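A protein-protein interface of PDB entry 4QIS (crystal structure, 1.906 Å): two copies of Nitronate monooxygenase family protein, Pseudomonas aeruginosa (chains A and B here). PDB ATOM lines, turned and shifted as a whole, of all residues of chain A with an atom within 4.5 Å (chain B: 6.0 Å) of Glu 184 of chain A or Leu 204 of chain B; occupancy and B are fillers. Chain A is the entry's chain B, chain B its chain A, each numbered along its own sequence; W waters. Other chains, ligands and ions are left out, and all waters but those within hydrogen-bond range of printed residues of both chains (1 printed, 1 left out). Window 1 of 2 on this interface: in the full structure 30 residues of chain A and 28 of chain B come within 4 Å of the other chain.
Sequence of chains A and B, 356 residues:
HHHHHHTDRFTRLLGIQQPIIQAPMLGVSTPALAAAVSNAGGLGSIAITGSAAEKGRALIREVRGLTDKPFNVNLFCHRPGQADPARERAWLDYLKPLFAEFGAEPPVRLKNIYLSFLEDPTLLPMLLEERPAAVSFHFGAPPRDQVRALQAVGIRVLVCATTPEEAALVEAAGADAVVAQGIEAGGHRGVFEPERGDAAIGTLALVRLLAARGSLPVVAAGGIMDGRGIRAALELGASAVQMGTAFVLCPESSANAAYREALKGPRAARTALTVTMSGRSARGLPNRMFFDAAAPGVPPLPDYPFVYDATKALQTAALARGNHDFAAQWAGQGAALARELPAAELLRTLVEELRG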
ATOM      1  N   GLY A 182       0.542 -22.616  19.378  1.00  0.00           N
ATOM      2  CA  GLY A 182      -0.670 -22.426  18.597  1.00  0.00           C
ATOM      3  C   GLY A 182      -1.540 -23.669  18.698  1.00  0.00           C
ATOM      4  O   GLY A 182      -1.085 -24.697  19.217  1.00  0.00           O
ATOM      5  N   ILE A 183      -2.759 -23.582  18.182  1.00  0.00           N
ATOM      6  CA  ILE A 183      -3.741 -24.660  18.224  1.00  0.00           C
ATOM      7  C   ILE A 183      -3.208 -25.918  17.516  1.00  0.00           C
ATOM      8  O   ILE A 183      -3.627 -27.026  17.818  1.00  0.00           O
ATOM      9  CB  ILE A 183      -5.096 -24.222  17.576  1.00  0.00           C
ATOM     10  CG1 ILE A 183      -6.248 -25.110  18.030  1.00  0.00           C
ATOM     11  CG2 ILE A 183      -5.013 -24.221  16.050  1.00  0.00           C
ATOM     12  CD1 ILE A 183      -6.423 -25.156  19.554  1.00  0.00           C
ATOM     13  N   GLU A 184      -2.272 -25.740  16.593  1.00  0.00           N
ATOM     14  CA  GLU A 184      -1.723 -26.875  15.845  1.00  0.00           C
ATOM     15  C   GLU A 184      -0.996 -27.899  16.728  1.00  0.00           C
ATOM     16  O   GLU A 184      -0.957 -29.083  16.401  1.00  0.00           O
ATOM     17  CB  GLU A 184      -0.766 -26.387  14.765  1.00  0.00           C
ATOM     18  CG  GLU A 184      -1.454 -25.761  13.573  1.00  0.00           C
ATOM     19  CD  GLU A 184      -1.690 -24.260  13.718  1.00  0.00           C
ATOM     20  OE1 GLU A 184      -1.934 -23.768  14.833  1.00  0.00           O
ATOM     21  OE2 GLU A 184      -1.617 -23.570  12.688  1.00  0.00           O
ATOM     22  N   ALA A 185      -0.444 -27.425  17.842  1.00  0.00           N
ATOM     23  CA  ALA A 185       0.452 -28.209  18.700  1.00  0.00           C
ATOM     24  C   ALA A 185      -0.112 -29.536  19.175  1.00  0.00           C
ATOM     25  O   ALA A 185      -1.285 -29.630  19.554  1.00  0.00           O
ATOM     26  CB  ALA A 185       0.881 -27.379  19.899  1.00  0.00           C
ATOM     27  N   GLY A 186       0.740 -30.560  19.148  1.00  0.00           N
ATOM     28  CA  GLY A 186       0.398 -31.865  19.675  1.00  0.00           C
ATOM     29  C   GLY A 186       0.580 -31.871  21.181  1.00  0.00           C
ATOM     30  O   GLY A 186       1.288 -31.017  21.727  1.00  0.00           O
ATOM     31  N   GLY A 202      -4.432 -20.055  16.489  1.00  0.00           N
ATOM     32  CA  GLY A 202      -3.512 -20.744  15.604  1.00  0.00           C
ATOM     33  C   GLY A 202      -2.111 -20.167  15.704  1.00  0.00           C
ATOM     34  O   GLY A 202      -1.941 -18.984  16.026  1.00  0.00           O
ATOM     35  N   THR A 203      -1.112 -21.005  15.419  1.00  0.00           N
ATOM     36  CA  THR A 203       0.295 -20.594  15.418  1.00  0.00           C
ATOM     37  C   THR A 203       0.576 -19.307  14.644  1.00  0.00           C
ATOM     38  O   THR A 203       1.184 -18.380  15.195  1.00  0.00           O
ATOM     39  CB  THR A 203       1.217 -21.740  14.927  1.00  0.00           C
ATOM     40  OG1 THR A 203       1.000 -22.902  15.747  1.00  0.00           O
ATOM     41  CG2 THR A 203       2.686 -21.324  14.986  1.00  0.00           C
ATOM     42  N   LEU A 204       0.112 -19.228  13.395  1.00  0.00           N
ATOM     43  CA  LEU A 204       0.350 -18.043  12.570  1.00  0.00           C
ATOM     44  C   LEU A 204      -0.090 -16.759  13.283  1.00  0.00           C
ATOM     45  O   LEU A 204       0.674 -15.802  13.357  1.00  0.00           O
ATOM     46  CB  LEU A 204      -0.301 -18.166  11.176  1.00  0.00           C
ATOM     47  CG  LEU A 204      -0.074 -17.047  10.140  1.00  0.00           C
ATOM     48  CD1 LEU A 204       0.150 -17.624   8.728  1.00  0.00           C
ATOM     49  CD2 LEU A 204      -1.208 -16.025  10.095  1.00  0.00           C
ATOM     50  N   GLY A 222       3.920 -25.410  17.219  1.00  0.00           N
ATOM     51  CA  GLY A 222       2.673 -25.981  16.758  1.00  0.00           C
ATOM     52  C   GLY A 222       2.586 -26.052  15.245  1.00  0.00           C
ATOM     53  O   GLY A 222       2.469 -25.020  14.576  1.00  0.00           O
ATOM     54  N   GLY A 223       2.628 -27.271  14.706  1.00  0.00           N
ATOM     55  CA  GLY A 223       2.466 -27.478  13.276  1.00  0.00           C
ATOM     56  C   GLY A 223       3.738 -27.381  12.442  1.00  0.00           C
ATOM     57  O   GLY A 223       3.693 -27.569  11.236  1.00  0.00           O
ATOM     58  N   ILE A 224       4.868 -27.085  13.071  1.00  0.00           N
ATOM     59  CA  ILE A 224       6.121 -26.872  12.329  1.00  0.00           C
ATOM     60  C   ILE A 224       6.846 -28.207  12.090  1.00  0.00           C
ATOM     61  O   ILE A 224       7.225 -28.895  13.042  1.00  0.00           O
ATOM     62  CB  ILE A 224       7.034 -25.852  13.053  1.00  0.00           C
ATOM     63  CG1 ILE A 224       6.342 -24.479  13.112  1.00  0.00           C
ATOM     64  CG2 ILE A 224       8.358 -25.724  12.338  1.00  0.00           C
ATOM     65  CD1 ILE A 224       6.985 -23.479  14.065  1.00  0.00           C
ATOM     66  N   ARG A 283      -4.021 -32.746  22.329  1.00  0.00           N
ATOM     67  CA  ARG A 283      -4.266 -33.112  20.936  1.00  0.00           C
ATOM     68  C   ARG A 283      -3.497 -34.361  20.539  1.00  0.00           C
ATOM     69  O   ARG A 283      -2.291 -34.446  20.751  1.00  0.00           O
ATOM     70  CB  ARG A 283      -3.856 -31.977  19.995  1.00  0.00           C
ATOM     71  CG  ARG A 283      -3.915 -32.355  18.515  1.00  0.00           C
ATOM     72  CD  ARG A 283      -3.422 -31.223  17.589  1.00  0.00           C
ATOM     73  NE  ARG A 283      -4.170 -29.991  17.841  1.00  0.00           N
ATOM     74  CZ  ARG A 283      -5.409 -29.754  17.414  1.00  0.00           C
ATOM     75  NH1 ARG A 283      -6.057 -30.660  16.689  1.00  0.00           N
ATOM     76  NH2 ARG A 283      -6.004 -28.599  17.706  1.00  0.00           N
ATOM     77  N   GLY A 332       0.694 -33.244  16.497  1.00  0.00           N
ATOM     78  CA  GLY A 332       0.237 -31.926  16.101  1.00  0.00           C
ATOM     79  C   GLY A 332      -0.419 -31.980  14.744  1.00  0.00           C
ATOM     80  O   GLY A 332      -0.347 -33.013  14.065  1.00  0.00           O
ATOM     81  N   GLN A 333      -1.059 -30.879  14.342  1.00  0.00           N
ATOM     82  CA  GLN A 333      -1.821 -30.853  13.092  1.00  0.00           C
ATOM     83  C   GLN A 333      -0.976 -31.005  11.815  1.00  0.00           C
ATOM     84  O   GLN A 333      -1.531 -31.227  10.736  1.00  0.00           O
ATOM     85  CB  GLN A 333      -2.693 -29.604  13.004  1.00  0.00           C
ATOM     86  CG  GLN A 333      -3.853 -29.599  14.004  1.00  0.00           C
ATOM     87  CD  GLN A 333      -4.692 -28.340  13.904  1.00  0.00           C
ATOM     88  OE1 GLN A 333      -4.173 -27.279  13.573  1.00  0.00           O
ATOM     89  NE2 GLN A 333      -5.991 -28.456  14.178  1.00  0.00           N
ATOM     90  N   ILE B 183      -7.981 -21.885  10.989  1.00  0.00           N
ATOM     91  CA  ILE B 183      -8.858 -21.579  12.125  1.00  0.00           C
ATOM     92  C   ILE B 183      -8.869 -20.083  12.490  1.00  0.00           C
ATOM     93  O   ILE B 183      -9.852 -19.593  13.051  1.00  0.00           O
ATOM     94  CB  ILE B 183      -8.459 -22.410  13.375  1.00  0.00           C
ATOM     95  CG1 ILE B 183      -9.605 -22.494  14.387  1.00  0.00           C
ATOM     96  CG2 ILE B 183      -7.236 -21.809  14.042  1.00  0.00           C
ATOM     97  CD1 ILE B 183     -10.927 -22.997  13.817  1.00  0.00           C
ATOM     98  N   GLU B 184      -7.793 -19.373  12.132  1.00  0.00           N
ATOM     99  CA  GLU B 184      -7.631 -17.943  12.395  1.00  0.00           C
ATOM    100  C   GLU B 184      -8.680 -17.103  11.719  1.00  0.00           C
ATOM    101  O   GLU B 184      -8.926 -15.969  12.121  1.00  0.00           O
ATOM    102  CB  GLU B 184      -6.266 -17.451  11.889  1.00  0.00           C
ATOM    103  CG  GLU B 184      -5.077 -17.813  12.758  1.00  0.00           C
ATOM    104  CD  GLU B 184      -4.443 -19.176  12.442  1.00  0.00           C
ATOM    105  OE1 GLU B 184      -5.139 -20.100  11.956  1.00  0.00           O
ATOM    106  OE2 GLU B 184      -3.234 -19.327  12.693  1.00  0.00           O
ATOM    107  N   ILE B 201      -8.257 -26.799  11.781  1.00  0.00           N
ATOM    108  CA  ILE B 201      -6.825 -26.662  11.520  1.00  0.00           C
ATOM    109  C   ILE B 201      -6.348 -25.209  11.368  1.00  0.00           C
ATOM    110  O   ILE B 201      -6.982 -24.406  10.681  1.00  0.00           O
ATOM    111  CB  ILE B 201      -6.459 -27.441  10.248  1.00  0.00           C
ATOM    112  CG1 ILE B 201      -6.950 -28.887  10.404  1.00  0.00           C
ATOM    113  CG2 ILE B 201      -4.959 -27.377  10.003  1.00  0.00           C
ATOM    114  CD1 ILE B 201      -6.939 -29.710   9.119  1.00  0.00           C
ATOM    115  N   GLY B 202      -5.214 -24.887  11.993  1.00  0.00           N
ATOM    116  CA  GLY B 202      -4.629 -23.561  11.902  1.00  0.00           C
ATOM    117  C   GLY B 202      -4.027 -23.294  10.532  1.00  0.00           C
ATOM    118  O   GLY B 202      -3.662 -24.222   9.817  1.00  0.00           O
ATOM    119  N   THR B 203      -3.931 -22.023  10.165  1.00  0.00           N
ATOM    120  CA  THR B 203      -3.419 -21.634   8.854  1.00  0.00           C
ATOM    121  C   THR B 203      -2.039 -22.226   8.580  1.00  0.00           C
ATOM    122  O   THR B 203      -1.794 -22.753   7.494  1.00  0.00           O
ATOM    123  CB  THR B 203      -3.356 -20.100   8.709  1.00  0.00           C
ATOM    124  OG1 THR B 203      -4.667 -19.567   8.868  1.00  0.00           O
ATOM    125  CG2 THR B 203      -2.828 -19.687   7.318  1.00  0.00           C
ATOM    126  N   LEU B 204      -1.154 -22.156   9.574  1.00  0.00           N
ATOM    127  CA  LEU B 204       0.210 -22.619   9.384  1.00  0.00           C
ATOM    128  C   LEU B 204       0.296 -24.091   8.973  1.00  0.00           C
ATOM    129  O   LEU B 204       1.037 -24.419   8.046  1.00  0.00           O
ATOM    130  CB  LEU B 204       1.110 -22.315  10.585  1.00  0.00           C
ATOM    131  CG  LEU B 204       2.581 -22.734  10.423  1.00  0.00           C
ATOM    132  CD1 LEU B 204       3.561 -21.656  10.851  1.00  0.00           C
ATOM    133  CD2 LEU B 204       2.859 -24.009  11.188  1.00  0.00           C
ATOM    134  N   ALA B 205      -0.459 -24.966   9.643  1.00  0.00           N
ATOM    135  CA  ALA B 205      -0.502 -26.379   9.251  1.00  0.00           C
ATOM    136  C   ALA B 205      -1.220 -26.595   7.912  1.00  0.00           C
ATOM    137  O   ALA B 205      -0.700 -27.286   7.032  1.00  0.00           O
ATOM    138  CB  ALA B 205      -1.153 -27.232  10.334  1.00  0.00           C
ATOM    139  N   LEU B 206      -2.407 -26.008   7.774  1.00  0.00           N
ATOM    140  CA  LEU B 206      -3.249 -26.214   6.602  1.00  0.00           C
ATOM    141  C   LEU B 206      -2.578 -25.809   5.291  1.00  0.00           C
ATOM    142  O   LEU B 206      -2.625 -26.563   4.322  1.00  0.00           O
ATOM    143  CB  LEU B 206      -4.588 -25.490   6.756  1.00  0.00           C
ATOM    144  CG  LEU B 206      -5.577 -25.726   5.607  1.00  0.00           C
ATOM    145  CD1 LEU B 206      -6.011 -27.187   5.554  1.00  0.00           C
ATOM    146  CD2 LEU B 206      -6.799 -24.820   5.710  1.00  0.00           C
ATOM    147  N   VAL B 207      -1.964 -24.630   5.250  1.00  0.00           N
ATOM    148  CA  VAL B 207      -1.298 -24.195   4.024  1.00  0.00           C
ATOM    149  C   VAL B 207      -0.173 -25.151   3.653  1.00  0.00           C
ATOM    150  O   VAL B 207      -0.042 -25.539   2.495  1.00  0.00           O
ATOM    151  CB  VAL B 207      -0.686 -22.786   4.148  1.00  0.00           C
ATOM    152  CG1 VAL B 207       0.106 -22.446   2.878  1.00  0.00           C
ATOM    153  CG2 VAL B 207      -1.774 -21.731   4.444  1.00  0.00           C
ATOM    154  N   ARG B 208       0.626 -25.532   4.648  1.00  0.00           N
ATOM    155  CA  ARG B 208       1.765 -26.404   4.409  1.00  0.00           C
ATOM    156  C   ARG B 208       1.302 -27.727   3.856  1.00  0.00           C
ATOM    157  O   ARG B 208       1.865 -28.234   2.894  1.00  0.00           O
ATOM    158  CB  ARG B 208       2.591 -26.622   5.673  1.00  0.00           C
ATOM    159  CG  ARG B 208       3.949 -27.266   5.379  1.00  0.00           C
ATOM    160  CD  ARG B 208       4.868 -26.274   4.648  1.00  0.00           C
ATOM    161  NE  ARG B 208       5.953 -26.959   3.961  1.00  0.00           N
ATOM    162  CZ  ARG B 208       5.968 -27.208   2.655  1.00  0.00           C
ATOM    163  NH1 ARG B 208       6.985 -27.861   2.122  1.00  0.00           N
ATOM    164  NH2 ARG B 208       4.972 -26.802   1.880  1.00  0.00           N
ATOM    165  N   LEU B 209       0.255 -28.269   4.454  1.00  0.00           N
ATOM    166  CA  LEU B 209      -0.302 -29.536   4.013  1.00  0.00           C
ATOM    167  C   LEU B 209      -0.734 -29.484   2.547  1.00  0.00           C
ATOM    168  O   LEU B 209      -0.342 -30.337   1.754  1.00  0.00           O
ATOM    169  CB  LEU B 209      -1.468 -29.943   4.914  1.00  0.00           C
ATOM    170  CG  LEU B 209      -1.045 -30.339   6.339  1.00  0.00           C
ATOM    171  CD1 LEU B 209      -2.252 -30.597   7.223  1.00  0.00           C
ATOM    172  CD2 LEU B 209      -0.119 -31.556   6.330  1.00  0.00           C
ATOM    173  N   LEU B 236       5.384 -20.991   3.385  1.00  0.00           N
ATOM    174  CA  LEU B 236       4.651 -22.247   3.603  1.00  0.00           C
ATOM    175  C   LEU B 236       4.210 -22.913   2.309  1.00  0.00           C
ATOM    176  O   LEU B 236       3.699 -24.033   2.332  1.00  0.00           O
ATOM    177  CB  LEU B 236       3.419 -22.017   4.480  1.00  0.00           C
ATOM    178  CG  LEU B 236       3.642 -21.708   5.969  1.00  0.00           C
ATOM    179  CD1 LEU B 236       2.315 -21.396   6.690  1.00  0.00           C
ATOM    180  CD2 LEU B 236       4.359 -22.853   6.660  1.00  0.00           C
HETATM  181  O   HOH W   1       3.537 -26.307   8.711  1.00  0.00           O
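The side-chain carboxylate of Glu 184 of chain B sits at hydrogen-bond distance from the backbone NH of Leu 204 of chain A. The backbone NH (N) of Gly 202 of chain B lies within hydrogen-bond range of the side-chain amide oxygen (OE1) of Gln 333 of chain A (3.0 Å). The side-chain carboxylate (OE2) of Glu 184 of chain A sits at hydrogen-bond distance from the backbone NH (N) of Leu 204 of chain B (3.5 Å).
N of Ile 183 of chain B sits at hydrogen-bond distance from O of Ile 201 of chain B (2.7 Å). The guanidinium group (NH2) of Arg 283 of chain A lies within hydrogen-bond range of the backbone carbonyl oxygen (O) of Ile 183 of chain A (2.9 Å). OE1 of Glu 184 of chain A lies within hydrogen-bond range of N of Thr 203 of chain A (2.9 Å). The backbone NH of Gln 333 of chain A is in hydrogen-bond range of the backbone carbonyl oxygen of Glu 184 of chain A, 2.7 Å away. O of Gly 222 of chain A is in hydrogen-bond range of OG1 of Thr 203 of chain A (2.8 Å). The side-chain amide nitrogen of Gln 333 of chain A sits close to the guanidinium group of Arg 283 of chain A, 3.3 Å away.
CG2 of Ile 183 of chain A touches CG2 of Ile 183 of chain B (3.8 Å). Glu 184 of chain A touches Gly 202 of chain B. Glu 184 of chain A touches Thr 203 of chain B. Glu 184 of chain A touches Ala 205 of chain B (OE2 to N, 3.5 Å). Gly 202 of chain A touches Glu 184 of chain B. OE2 of Glu 184 of chain B touches N of Thr 203 of chain A, 3.8 Å away. Leu 204 of chain A touches Thr 203 of chain B (CD1 to CG2, 3.9 Å). Gly 222 of chain A touches Leu 204 of chain B. CA of Ile 201 of chain B touches NE2 of Gln 333 of chain A, at 3.3 Å. Leu 209 of chain B touches Gln 333 of chain A (CD1 to O, 3.6 Å).
Printed residues of chain B within 4 Å of Ile 183 of chain A: Ile 183 (3.8 Å). Glu 184 of chain A touches four residues of chain B. Of the printed residues of chain B, Leu 204 of chain A touches Glu 184 (3.4 Å) and Thr 203 (3.9 Å). Printed residues of chain B within 4 Å of Gly 222 of chain A: Leu 204. Of the printed residues of chain B, Gln 333 of chain A touches Ile 201, Gly 202, Ala 205 and Leu 209. Of the printed residues of chain A, Leu 204 of chain B touches Glu 184 (3.5 Å), Gly 222 (3.6 Å) and Gly 223 (3.7 Å). Printed residues of chain A within 4 Å of Leu 209 of chain B: Gln 333. The nearest printed residue of chain A that does not touch Leu 204 of chain B is Ile 224 of chain A (4.01 Å).
Hydrophobic or aromatic side chains of chain A that line the printed part of chain B: Ile 183 and Leu 204. Hydrophobic or aromatic side chains of chain B that line the printed part of chain A: Ile 183, Ile 201, Leu 204, Ala 205 and Leu 209. Among the printed residues, no Asp or Glu carboxylate lies within 4 Å of a Lys or Arg side-chain nitrogen of the other chain.
Ile 183 of chain B touches its own counterpart, Ile 183 of chain A. Glu 184 of chain A touches Gly 202 of chain B, and with the chains exchanged Gly 202 of chain A touches Glu 184 of chain B. Glu 184 of chain A touches Thr 203 of chain B, and with the chains exchanged Thr 203 of chain A touches Glu 184 of chain B. Glu 184 of chain A touches Leu 204 of chain B, and with the chains exchanged Leu 204 of chain A touches Glu 184 of chain B. 5 positions are printed for both chains. Of the 15 pairs that touch across the chains among the printed residues, 7 have their exchanged pair printed and touching as well.
Water W1 lies within hydrogen-bond range of the backbone carbonyl oxygen of Gly 223 of chain A (2.8 Å) and the backbone carbonyl oxygen of Leu 204 of chain B (3.2 Å).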
